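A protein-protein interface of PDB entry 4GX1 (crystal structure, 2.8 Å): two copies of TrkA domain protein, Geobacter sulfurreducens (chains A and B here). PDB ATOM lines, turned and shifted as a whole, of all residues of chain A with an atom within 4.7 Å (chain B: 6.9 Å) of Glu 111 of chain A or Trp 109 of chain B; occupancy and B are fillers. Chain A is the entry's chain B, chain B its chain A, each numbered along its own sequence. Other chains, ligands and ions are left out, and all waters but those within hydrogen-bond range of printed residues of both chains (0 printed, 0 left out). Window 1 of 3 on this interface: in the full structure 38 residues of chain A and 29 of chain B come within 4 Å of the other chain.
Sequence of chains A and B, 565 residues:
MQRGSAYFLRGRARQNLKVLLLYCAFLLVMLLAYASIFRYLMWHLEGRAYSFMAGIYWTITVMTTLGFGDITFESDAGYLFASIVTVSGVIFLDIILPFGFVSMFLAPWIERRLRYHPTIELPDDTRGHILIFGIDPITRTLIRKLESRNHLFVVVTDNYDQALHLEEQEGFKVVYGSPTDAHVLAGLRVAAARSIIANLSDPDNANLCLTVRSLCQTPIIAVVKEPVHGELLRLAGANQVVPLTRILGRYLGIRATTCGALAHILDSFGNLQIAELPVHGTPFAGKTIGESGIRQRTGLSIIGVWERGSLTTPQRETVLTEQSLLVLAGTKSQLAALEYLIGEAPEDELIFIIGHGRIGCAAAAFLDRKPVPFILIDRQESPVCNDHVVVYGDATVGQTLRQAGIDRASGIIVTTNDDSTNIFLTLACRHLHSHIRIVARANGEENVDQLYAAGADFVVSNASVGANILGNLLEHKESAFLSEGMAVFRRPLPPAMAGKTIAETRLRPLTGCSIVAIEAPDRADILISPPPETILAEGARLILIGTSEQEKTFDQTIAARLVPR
Among the printed residues, merely in contact across the chains: Ala 107 of chain A with Trp 109 of chain B (3.8 Å), Ile 110 of chain A with Trp 109 of chain B (3.4 Å), Ile 110 of chain A with Leu 114 of chain B (3.9 Å) and Arg 115 of chain A with Arg 113 of chain B (3.5 Å).
NE1 of Trp 109 of chain B is in hydrogen-bond range of OE2 of Glu 111 of chain A (3.3 Å).
Ile 110 of chain A touches Trp 109 of chain B, but with the chains exchanged Trp 109 of chain A does not touch Ile 110 of chain B (11.3 Å).
Ile 110 of chain A touches Leu 114 of chain B, but with the chains exchanged Leu 114 of chain A does not touch Ile 110 of chain B (8.3 Å).
Glu 111 of chain A touches Trp 109 of chain B, but with the chains exchanged Trp 109 of chain A does not touch Glu 111 of chain B (14.1 Å).
Arg 115 of chain A touches Arg 113 of chain B, but with the chains exchanged Arg 113 of chain A does not touch Arg 115 of chain B (10.2 Å).
Positions printed for both chains: 107, 108, 109, 110, 111, 112, 113, 114 and 115.
Hydrophobic or aromatic side chains of chain A that line the printed part of chain B: Ala 107 and Ile 110.
Along chain A the printed residues that touch a printed residue of chain B span positions 107 to 115.
Of the 12 printed residues of chain B, 3 touch a printed residue of chain A.
Hydrophobic or aromatic side chains of chain B within 4 Å of the printed part of chain A: Trp 109 and Leu 114.
Among the printed residues, no Asp or Glu carboxylate lies within 4 Å of a Lys or Arg side-chain nitrogen of the other chain.
Of the printed residues of chain B, Glu 111 of chain A touches Trp 109.
Of the printed residues of chain A, Trp 109 of chain B touches Ala 107, Ile 110 and Glu 111.
Of the printed residues of chain B, Ile 110 of chain A touches Trp 109 (3.4 Å) and Leu 114 (3.9 Å).
Of the printed residues of chain A, Leu 114 of chain B touches Ile 110 (3.9 Å).
Glu 111 of chain B touches none of the printed residues of chain A.
The nearest residue of chain B that does not touch Glu 111 of chain A is Leu 114 of chain B (4.1 Å).
The nearest printed residue of chain A that does not touch Leu 114 of chain B is Glu 111 of chain A (4.1 Å).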
ATOM      1  N   ALA A 107       9.916   2.846  10.085  1.00  0.00           N
ATOM      2  CA  ALA A 107       8.576   3.425  10.151  1.00  0.00           C
ATOM      3  C   ALA A 107       7.463   2.547   9.549  1.00  0.00           C
ATOM      4  O   ALA A 107       6.414   2.385  10.170  1.00  0.00           O
ATOM      5  CB  ALA A 107       8.554   4.837   9.555  1.00  0.00           C
ATOM      6  N   PRO A 108       7.679   1.980   8.345  1.00  0.00           N
ATOM      7  CA  PRO A 108       6.635   1.092   7.815  1.00  0.00           C
ATOM      8  C   PRO A 108       6.387  -0.128   8.695  1.00  0.00           C
ATOM      9  O   PRO A 108       5.235  -0.496   8.899  1.00  0.00           O
ATOM     10  CB  PRO A 108       7.205   0.647   6.466  1.00  0.00           C
ATOM     11  CG  PRO A 108       8.120   1.745   6.070  1.00  0.00           C
ATOM     12  CD  PRO A 108       8.739   2.221   7.348  1.00  0.00           C
ATOM     13  N   TRP A 109       7.445  -0.741   9.209  1.00  0.00           N
ATOM     14  CA  TRP A 109       7.283  -1.927  10.040  1.00  0.00           C
ATOM     15  C   TRP A 109       6.577  -1.600  11.348  1.00  0.00           C
ATOM     16  O   TRP A 109       5.638  -2.294  11.741  1.00  0.00           O
ATOM     17  CB  TRP A 109       8.627  -2.602  10.323  1.00  0.00           C
ATOM     18  CG  TRP A 109       8.483  -3.854  11.141  1.00  0.00           C
ATOM     19  CD1 TRP A 109       8.020  -5.066  10.710  1.00  0.00           C
ATOM     20  CD2 TRP A 109       8.796  -4.016  12.529  1.00  0.00           C
ATOM     21  NE1 TRP A 109       8.027  -5.971  11.744  1.00  0.00           N
ATOM     22  CE2 TRP A 109       8.499  -5.352  12.872  1.00  0.00           C
ATOM     23  CE3 TRP A 109       9.299  -3.163  13.516  1.00  0.00           C
ATOM     24  CZ2 TRP A 109       8.691  -5.854  14.158  1.00  0.00           C
ATOM     25  CZ3 TRP A 109       9.487  -3.663  14.793  1.00  0.00           C
ATOM     26  CH2 TRP A 109       9.183  -4.996  15.101  1.00  0.00           C
ATOM     27  N   ILE A 110       7.027  -0.542  12.015  1.00  0.00           N
ATOM     28  CA  ILE A 110       6.443  -0.136  13.291  1.00  0.00           C
ATOM     29  C   ILE A 110       4.956   0.216  13.152  1.00  0.00           C
ATOM     30  O   ILE A 110       4.153  -0.096  14.032  1.00  0.00           O
ATOM     31  CB  ILE A 110       7.231   1.025  13.940  1.00  0.00           C
ATOM     32  CG1 ILE A 110       8.612   0.542  14.381  1.00  0.00           C
ATOM     33  CG2 ILE A 110       6.496   1.567  15.152  1.00  0.00           C
ATOM     34  CD1 ILE A 110       8.572  -0.415  15.556  1.00  0.00           C
ATOM     35  N   GLU A 111       4.589   0.845  12.040  1.00  0.00           N
ATOM     36  CA  GLU A 111       3.187   1.142  11.766  1.00  0.00           C
ATOM     37  C   GLU A 111       2.359  -0.130  11.623  1.00  0.00           C
ATOM     38  O   GLU A 111       1.347  -0.293  12.297  1.00  0.00           O
ATOM     39  CB  GLU A 111       3.042   1.995  10.508  1.00  0.00           C
ATOM     40  CG  GLU A 111       3.458   3.439  10.688  1.00  0.00           C
ATOM     41  CD  GLU A 111       3.365   4.230   9.398  1.00  0.00           C
ATOM     42  OE1 GLU A 111       2.266   4.257   8.796  1.00  0.00           O
ATOM     43  OE2 GLU A 111       4.395   4.812   8.985  1.00  0.00           O
ATOM     44  N   ARG A 112       2.794  -1.032  10.749  1.00  0.00           N
ATOM     45  CA  ARG A 112       2.065  -2.272  10.510  1.00  0.00           C
ATOM     46  C   ARG A 112       2.023  -3.169  11.744  1.00  0.00           C
ATOM     47  O   ARG A 112       1.186  -4.069  11.832  1.00  0.00           O
ATOM     48  CB  ARG A 112       2.681  -3.056   9.349  1.00  0.00           C
ATOM     49  CG  ARG A 112       2.784  -2.297   8.039  1.00  0.00           C
ATOM     50  CD  ARG A 112       1.456  -1.682   7.624  1.00  0.00           C
ATOM     51  NE  ARG A 112       1.181  -1.853   6.198  1.00  0.00           N
ATOM     52  CZ  ARG A 112       1.843  -1.242   5.217  1.00  0.00           C
ATOM     53  NH1 ARG A 112       2.842  -0.410   5.492  1.00  0.00           N
ATOM     54  NH2 ARG A 112       1.506  -1.472   3.954  1.00  0.00           N
ATOM     55  N   ARG A 113       2.925  -2.931  12.691  1.00  0.00           N
ATOM     56  CA  ARG A 113       3.036  -3.802  13.857  1.00  0.00           C
ATOM     57  C   ARG A 113       2.442  -3.189  15.130  1.00  0.00           C
ATOM     58  O   ARG A 113       2.277  -3.875  16.139  1.00  0.00           O
ATOM     59  CB  ARG A 113       4.495  -4.209  14.084  1.00  0.00           C
ATOM     60  CG  ARG A 113       4.658  -5.610  14.649  1.00  0.00           C
ATOM     61  CD  ARG A 113       5.371  -6.532  13.669  1.00  0.00           C
ATOM     62  NE  ARG A 113       4.693  -6.621  12.378  1.00  0.00           N
ATOM     63  CZ  ARG A 113       3.802  -7.558  12.061  1.00  0.00           C
ATOM     64  NH1 ARG A 113       3.474  -8.490  12.945  1.00  0.00           N
ATOM     65  NH2 ARG A 113       3.240  -7.562  10.859  1.00  0.00           N
ATOM     66  N   LEU A 114       2.116  -1.902  15.078  1.00  0.00           N
ATOM     67  CA  LEU A 114       1.500  -1.228  16.218  1.00  0.00           C
ATOM     68  C   LEU A 114       0.071  -0.797  15.923  1.00  0.00           C
ATOM     69  O   LEU A 114      -0.725  -0.576  16.833  1.00  0.00           O
ATOM     70  CB  LEU A 114       2.315  -0.004  16.630  1.00  0.00           C
ATOM     71  CG  LEU A 114       3.384  -0.267  17.684  1.00  0.00           C
ATOM     72  CD1 LEU A 114       2.808  -1.127  18.799  1.00  0.00           C
ATOM     73  CD2 LEU A 114       4.603  -0.918  17.062  1.00  0.00           C
ATOM     74  N   ARG A 115      -0.242  -0.679  14.640  1.00  0.00           N
ATOM     75  CA  ARG A 115      -1.521  -0.152  14.202  1.00  0.00           C
ATOM     76  C   ARG A 115      -2.016  -0.963  13.018  1.00  0.00           C
ATOM     77  O   ARG A 115      -1.314  -1.089  12.017  1.00  0.00           O
ATOM     78  CB  ARG A 115      -1.354   1.311  13.792  1.00  0.00           C
ATOM     79  CG  ARG A 115      -2.535   1.893  13.049  1.00  0.00           C
ATOM     80  CD  ARG A 115      -3.444   2.670  13.980  1.00  0.00           C
ATOM     81  NE  ARG A 115      -3.435   4.095  13.668  1.00  0.00           N
ATOM     82  CZ  ARG A 115      -4.246   4.985  14.228  1.00  0.00           C
ATOM     83  NH1 ARG A 115      -5.133   4.592  15.133  1.00  0.00           N
ATOM     84  NH2 ARG A 115      -4.172   6.265  13.881  1.00  0.00           N
ATOM     85  N   HIS A 117      -3.586  -1.599   9.696  1.00  0.00           N
ATOM     86  CA  HIS A 117      -3.965  -0.901   8.474  1.00  0.00           C
ATOM     87  C   HIS A 117      -4.774  -1.848   7.595  1.00  0.00           C
ATOM     88  O   HIS A 117      -4.227  -2.796   7.029  1.00  0.00           O
ATOM     89  CB  HIS A 117      -2.730  -0.402   7.723  1.00  0.00           C
ATOM     90  CG  HIS A 117      -1.900   0.570   8.504  1.00  0.00           C
ATOM     91  ND1 HIS A 117      -2.153   1.925   8.513  1.00  0.00           N
ATOM     92  CD2 HIS A 117      -0.820   0.384   9.299  1.00  0.00           C
ATOM     93  CE1 HIS A 117      -1.265   2.531   9.281  1.00  0.00           C
ATOM     94  NE2 HIS A 117      -0.445   1.619   9.771  1.00  0.00           N
ATOM     95  N   MET B 104      12.070  16.406  17.271  1.00  0.00           N
ATOM     96  CA  MET B 104      11.316  17.360  16.463  1.00  0.00           C
ATOM     97  C   MET B 104      10.330  16.697  15.504  1.00  0.00           C
ATOM     98  O   MET B 104       9.186  17.139  15.406  1.00  0.00           O
ATOM     99  CB  MET B 104      12.249  18.324  15.718  1.00  0.00           C
ATOM    100  CG  MET B 104      11.700  18.866  14.411  1.00  0.00           C
ATOM    101  SD  MET B 104      12.955  19.771  13.489  1.00  0.00           S
ATOM    102  CE  MET B 104      12.596  19.227  11.821  1.00  0.00           C
ATOM    103  N   PHE B 105      10.747  15.649  14.797  1.00  0.00           N
ATOM    104  CA  PHE B 105       9.812  15.020  13.862  1.00  0.00           C
ATOM    105  C   PHE B 105       9.766  13.486  13.773  1.00  0.00           C
ATOM    106  O   PHE B 105       9.205  12.936  12.826  1.00  0.00           O
ATOM    107  CB  PHE B 105       9.835  15.695  12.477  1.00  0.00           C
ATOM    108  CG  PHE B 105      10.916  15.205  11.553  1.00  0.00           C
ATOM    109  CD1 PHE B 105      10.644  14.228  10.607  1.00  0.00           C
ATOM    110  CD2 PHE B 105      12.183  15.758  11.592  1.00  0.00           C
ATOM    111  CE1 PHE B 105      11.620  13.787   9.744  1.00  0.00           C
ATOM    112  CE2 PHE B 105      13.168  15.325  10.725  1.00  0.00           C
ATOM    113  CZ  PHE B 105      12.885  14.337   9.798  1.00  0.00           C
ATOM    114  N   LEU B 106      10.309  12.794  14.767  1.00  0.00           N
ATOM    115  CA  LEU B 106       9.994  11.373  14.919  1.00  0.00           C
ATOM    116  C   LEU B 106       8.879  11.218  15.955  1.00  0.00           C
ATOM    117  O   LEU B 106       8.130  10.242  15.945  1.00  0.00           O
ATOM    118  CB  LEU B 106      11.219  10.558  15.329  1.00  0.00           C
ATOM    119  CG  LEU B 106      11.066   9.039  15.192  1.00  0.00           C
ATOM    120  CD1 LEU B 106      11.213   8.605  13.733  1.00  0.00           C
ATOM    121  CD2 LEU B 106      12.048   8.299  16.097  1.00  0.00           C
ATOM    122  N   ALA B 107       8.781  12.198  16.847  1.00  0.00           N
ATOM    123  CA  ALA B 107       7.732  12.227  17.860  1.00  0.00           C
ATOM    124  C   ALA B 107       6.337  12.571  17.307  1.00  0.00           C
ATOM    125  O   ALA B 107       5.355  11.949  17.705  1.00  0.00           O
ATOM    126  CB  ALA B 107       8.119  13.160  19.014  1.00  0.00           C
ATOM    127  N   PRO B 108       6.237  13.567  16.400  1.00  0.00           N
ATOM    128  CA  PRO B 108       4.941  13.792  15.747  1.00  0.00           C
ATOM    129  C   PRO B 108       4.436  12.559  15.016  1.00  0.00           C
ATOM    130  O   PRO B 108       3.233  12.380  14.862  1.00  0.00           O
ATOM    131  CB  PRO B 108       5.257  14.882  14.720  1.00  0.00           C
ATOM    132  CG  PRO B 108       6.352  15.646  15.326  1.00  0.00           C
ATOM    133  CD  PRO B 108       7.181  14.660  16.102  1.00  0.00           C
ATOM    134  N   TRP B 109       5.360  11.721  14.566  1.00  0.00           N
ATOM    135  CA  TRP B 109       5.005  10.524  13.825  1.00  0.00           C
ATOM    136  C   TRP B 109       4.325   9.477  14.714  1.00  0.00           C
ATOM    137  O   TRP B 109       3.495   8.702  14.238  1.00  0.00           O
ATOM    138  CB  TRP B 109       6.241   9.956  13.124  1.00  0.00           C
ATOM    139  CG  TRP B 109       6.094   8.546  12.670  1.00  0.00           C
ATOM    140  CD1 TRP B 109       5.508   8.105  11.519  1.00  0.00           C
ATOM    141  CD2 TRP B 109       6.560   7.381  13.357  1.00  0.00           C
ATOM    142  NE1 TRP B 109       5.574   6.732  11.452  1.00  0.00           N
ATOM    143  CE2 TRP B 109       6.215   6.265  12.568  1.00  0.00           C
ATOM    144  CE3 TRP B 109       7.233   7.173  14.562  1.00  0.00           C
ATOM    145  CZ2 TRP B 109       6.522   4.961  12.952  1.00  0.00           C
ATOM    146  CZ3 TRP B 109       7.532   5.883  14.942  1.00  0.00           C
ATOM    147  CH2 TRP B 109       7.180   4.793  14.139  1.00  0.00           C
ATOM    148  N   ILE B 110       4.653   9.462  16.004  1.00  0.00           N
ATOM    149  CA  ILE B 110       4.015   8.516  16.920  1.00  0.00           C
ATOM    150  C   ILE B 110       2.635   8.999  17.375  1.00  0.00           C
ATOM    151  O   ILE B 110       1.687   8.219  17.438  1.00  0.00           O
ATOM    152  CB  ILE B 110       4.916   8.139  18.147  1.00  0.00           C
ATOM    153  CG1 ILE B 110       4.983   9.264  19.183  1.00  0.00           C
ATOM    154  CG2 ILE B 110       6.316   7.752  17.708  1.00  0.00           C
ATOM    155  CD1 ILE B 110       4.258   8.952  20.471  1.00  0.00           C
ATOM    156  N   GLU B 111       2.514  10.289  17.665  1.00  0.00           N
ATOM    157  CA  GLU B 111       1.262  10.822  18.183  1.00  0.00           C
ATOM    158  C   GLU B 111       0.241  11.054  17.076  1.00  0.00           C
ATOM    159  O   GLU B 111      -0.877  11.503  17.334  1.00  0.00           O
ATOM    160  CB  GLU B 111       1.498  12.114  18.974  1.00  0.00           C
ATOM    161  CG  GLU B 111       2.482  11.962  20.125  1.00  0.00           C
ATOM    162  CD  GLU B 111       2.232  12.942  21.256  1.00  0.00           C
ATOM    163  OE1 GLU B 111       1.075  13.388  21.417  1.00  0.00           O
ATOM    164  OE2 GLU B 111       3.198  13.263  21.985  1.00  0.00           O
ATOM    165  N   ARG B 112       0.620  10.736  15.843  1.00  0.00           N
ATOM    166  CA  ARG B 112      -0.279  10.938  14.717  1.00  0.00           C
ATOM    167  C   ARG B 112      -0.416   9.703  13.823  1.00  0.00           C
ATOM    168  O   ARG B 112      -1.230   9.695  12.899  1.00  0.00           O
ATOM    169  CB  ARG B 112       0.153  12.152  13.886  1.00  0.00           C
ATOM    170  CG  ARG B 112      -1.013  12.956  13.329  1.00  0.00           C
ATOM    171  CD  ARG B 112      -0.711  13.518  11.946  1.00  0.00           C
ATOM    172  NE  ARG B 112      -1.819  13.284  11.023  1.00  0.00           N
ATOM    173  CZ  ARG B 112      -1.770  13.518   9.715  1.00  0.00           C
ATOM    174  NH1 ARG B 112      -0.661  13.998   9.166  1.00  0.00           N
ATOM    175  NH2 ARG B 112      -2.829  13.270   8.955  1.00  0.00           N
ATOM    176  N   ARG B 113       0.367   8.661  14.094  1.00  0.00           N
ATOM    177  CA  ARG B 113       0.331   7.469  13.245  1.00  0.00           C
ATOM    178  C   ARG B 113       0.278   6.131  13.991  1.00  0.00           C
ATOM    179  O   ARG B 113      -0.094   5.108  13.414  1.00  0.00           O
ATOM    180  CB  ARG B 113       1.486   7.482  12.237  1.00  0.00           C
ATOM    181  CG  ARG B 113       1.357   8.563  11.172  1.00  0.00           C
ATOM    182  CD  ARG B 113       2.368   8.384  10.051  1.00  0.00           C
ATOM    183  NE  ARG B 113       1.809   8.737   8.746  1.00  0.00           N
ATOM    184  CZ  ARG B 113       2.020   9.890   8.116  1.00  0.00           C
ATOM    185  NH1 ARG B 113       2.789  10.822   8.665  1.00  0.00           N
ATOM    186  NH2 ARG B 113       1.462  10.107   6.932  1.00  0.00           N
ATOM    187  N   LEU B 114       0.642   6.134  15.268  1.00  0.00           N
ATOM    188  CA  LEU B 114       0.634   4.903  16.052  1.00  0.00           C
ATOM    189  C   LEU B 114      -0.515   4.931  17.049  1.00  0.00           C
ATOM    190  O   LEU B 114      -0.998   3.890  17.491  1.00  0.00           O
ATOM    191  CB  LEU B 114       1.964   4.718  16.786  1.00  0.00           C
ATOM    192  CG  LEU B 114       3.194   4.123  16.077  1.00  0.00           C
ATOM    193  CD1 LEU B 114       3.383   4.634  14.649  1.00  0.00           C
ATOM    194  CD2 LEU B 114       4.455   4.391  16.900  1.00  0.00           C
ATOM    195  N   ARG B 115      -0.951   6.138  17.395  1.00  0.00           N
ATOM    196  CA  ARG B 115      -2.066   6.341  18.312  1.00  0.00           C
ATOM    197  C   ARG B 115      -2.957   7.438  17.742  1.00  0.00           C
ATOM    198  O   ARG B 115      -2.547   8.597  17.679  1.00  0.00           O
ATOM    199  CB  ARG B 115      -1.544   6.754  19.688  1.00  0.00           C
ATOM    200  CG  ARG B 115      -2.480   6.447  20.849  1.00  0.00           C
ATOM    201  CD  ARG B 115      -2.511   4.955  21.166  1.00  0.00           C
ATOM    202  NE  ARG B 115      -2.964   4.697  22.531  1.00  0.00           N
ATOM    203  CZ  ARG B 115      -3.103   3.484  23.060  1.00  0.00           C
ATOM    204  NH1 ARG B 115      -2.827   2.406  22.340  1.00  0.00           N
ATOM    205  NH2 ARG B 115      -3.520   3.348  24.313  1.00  0.00           N
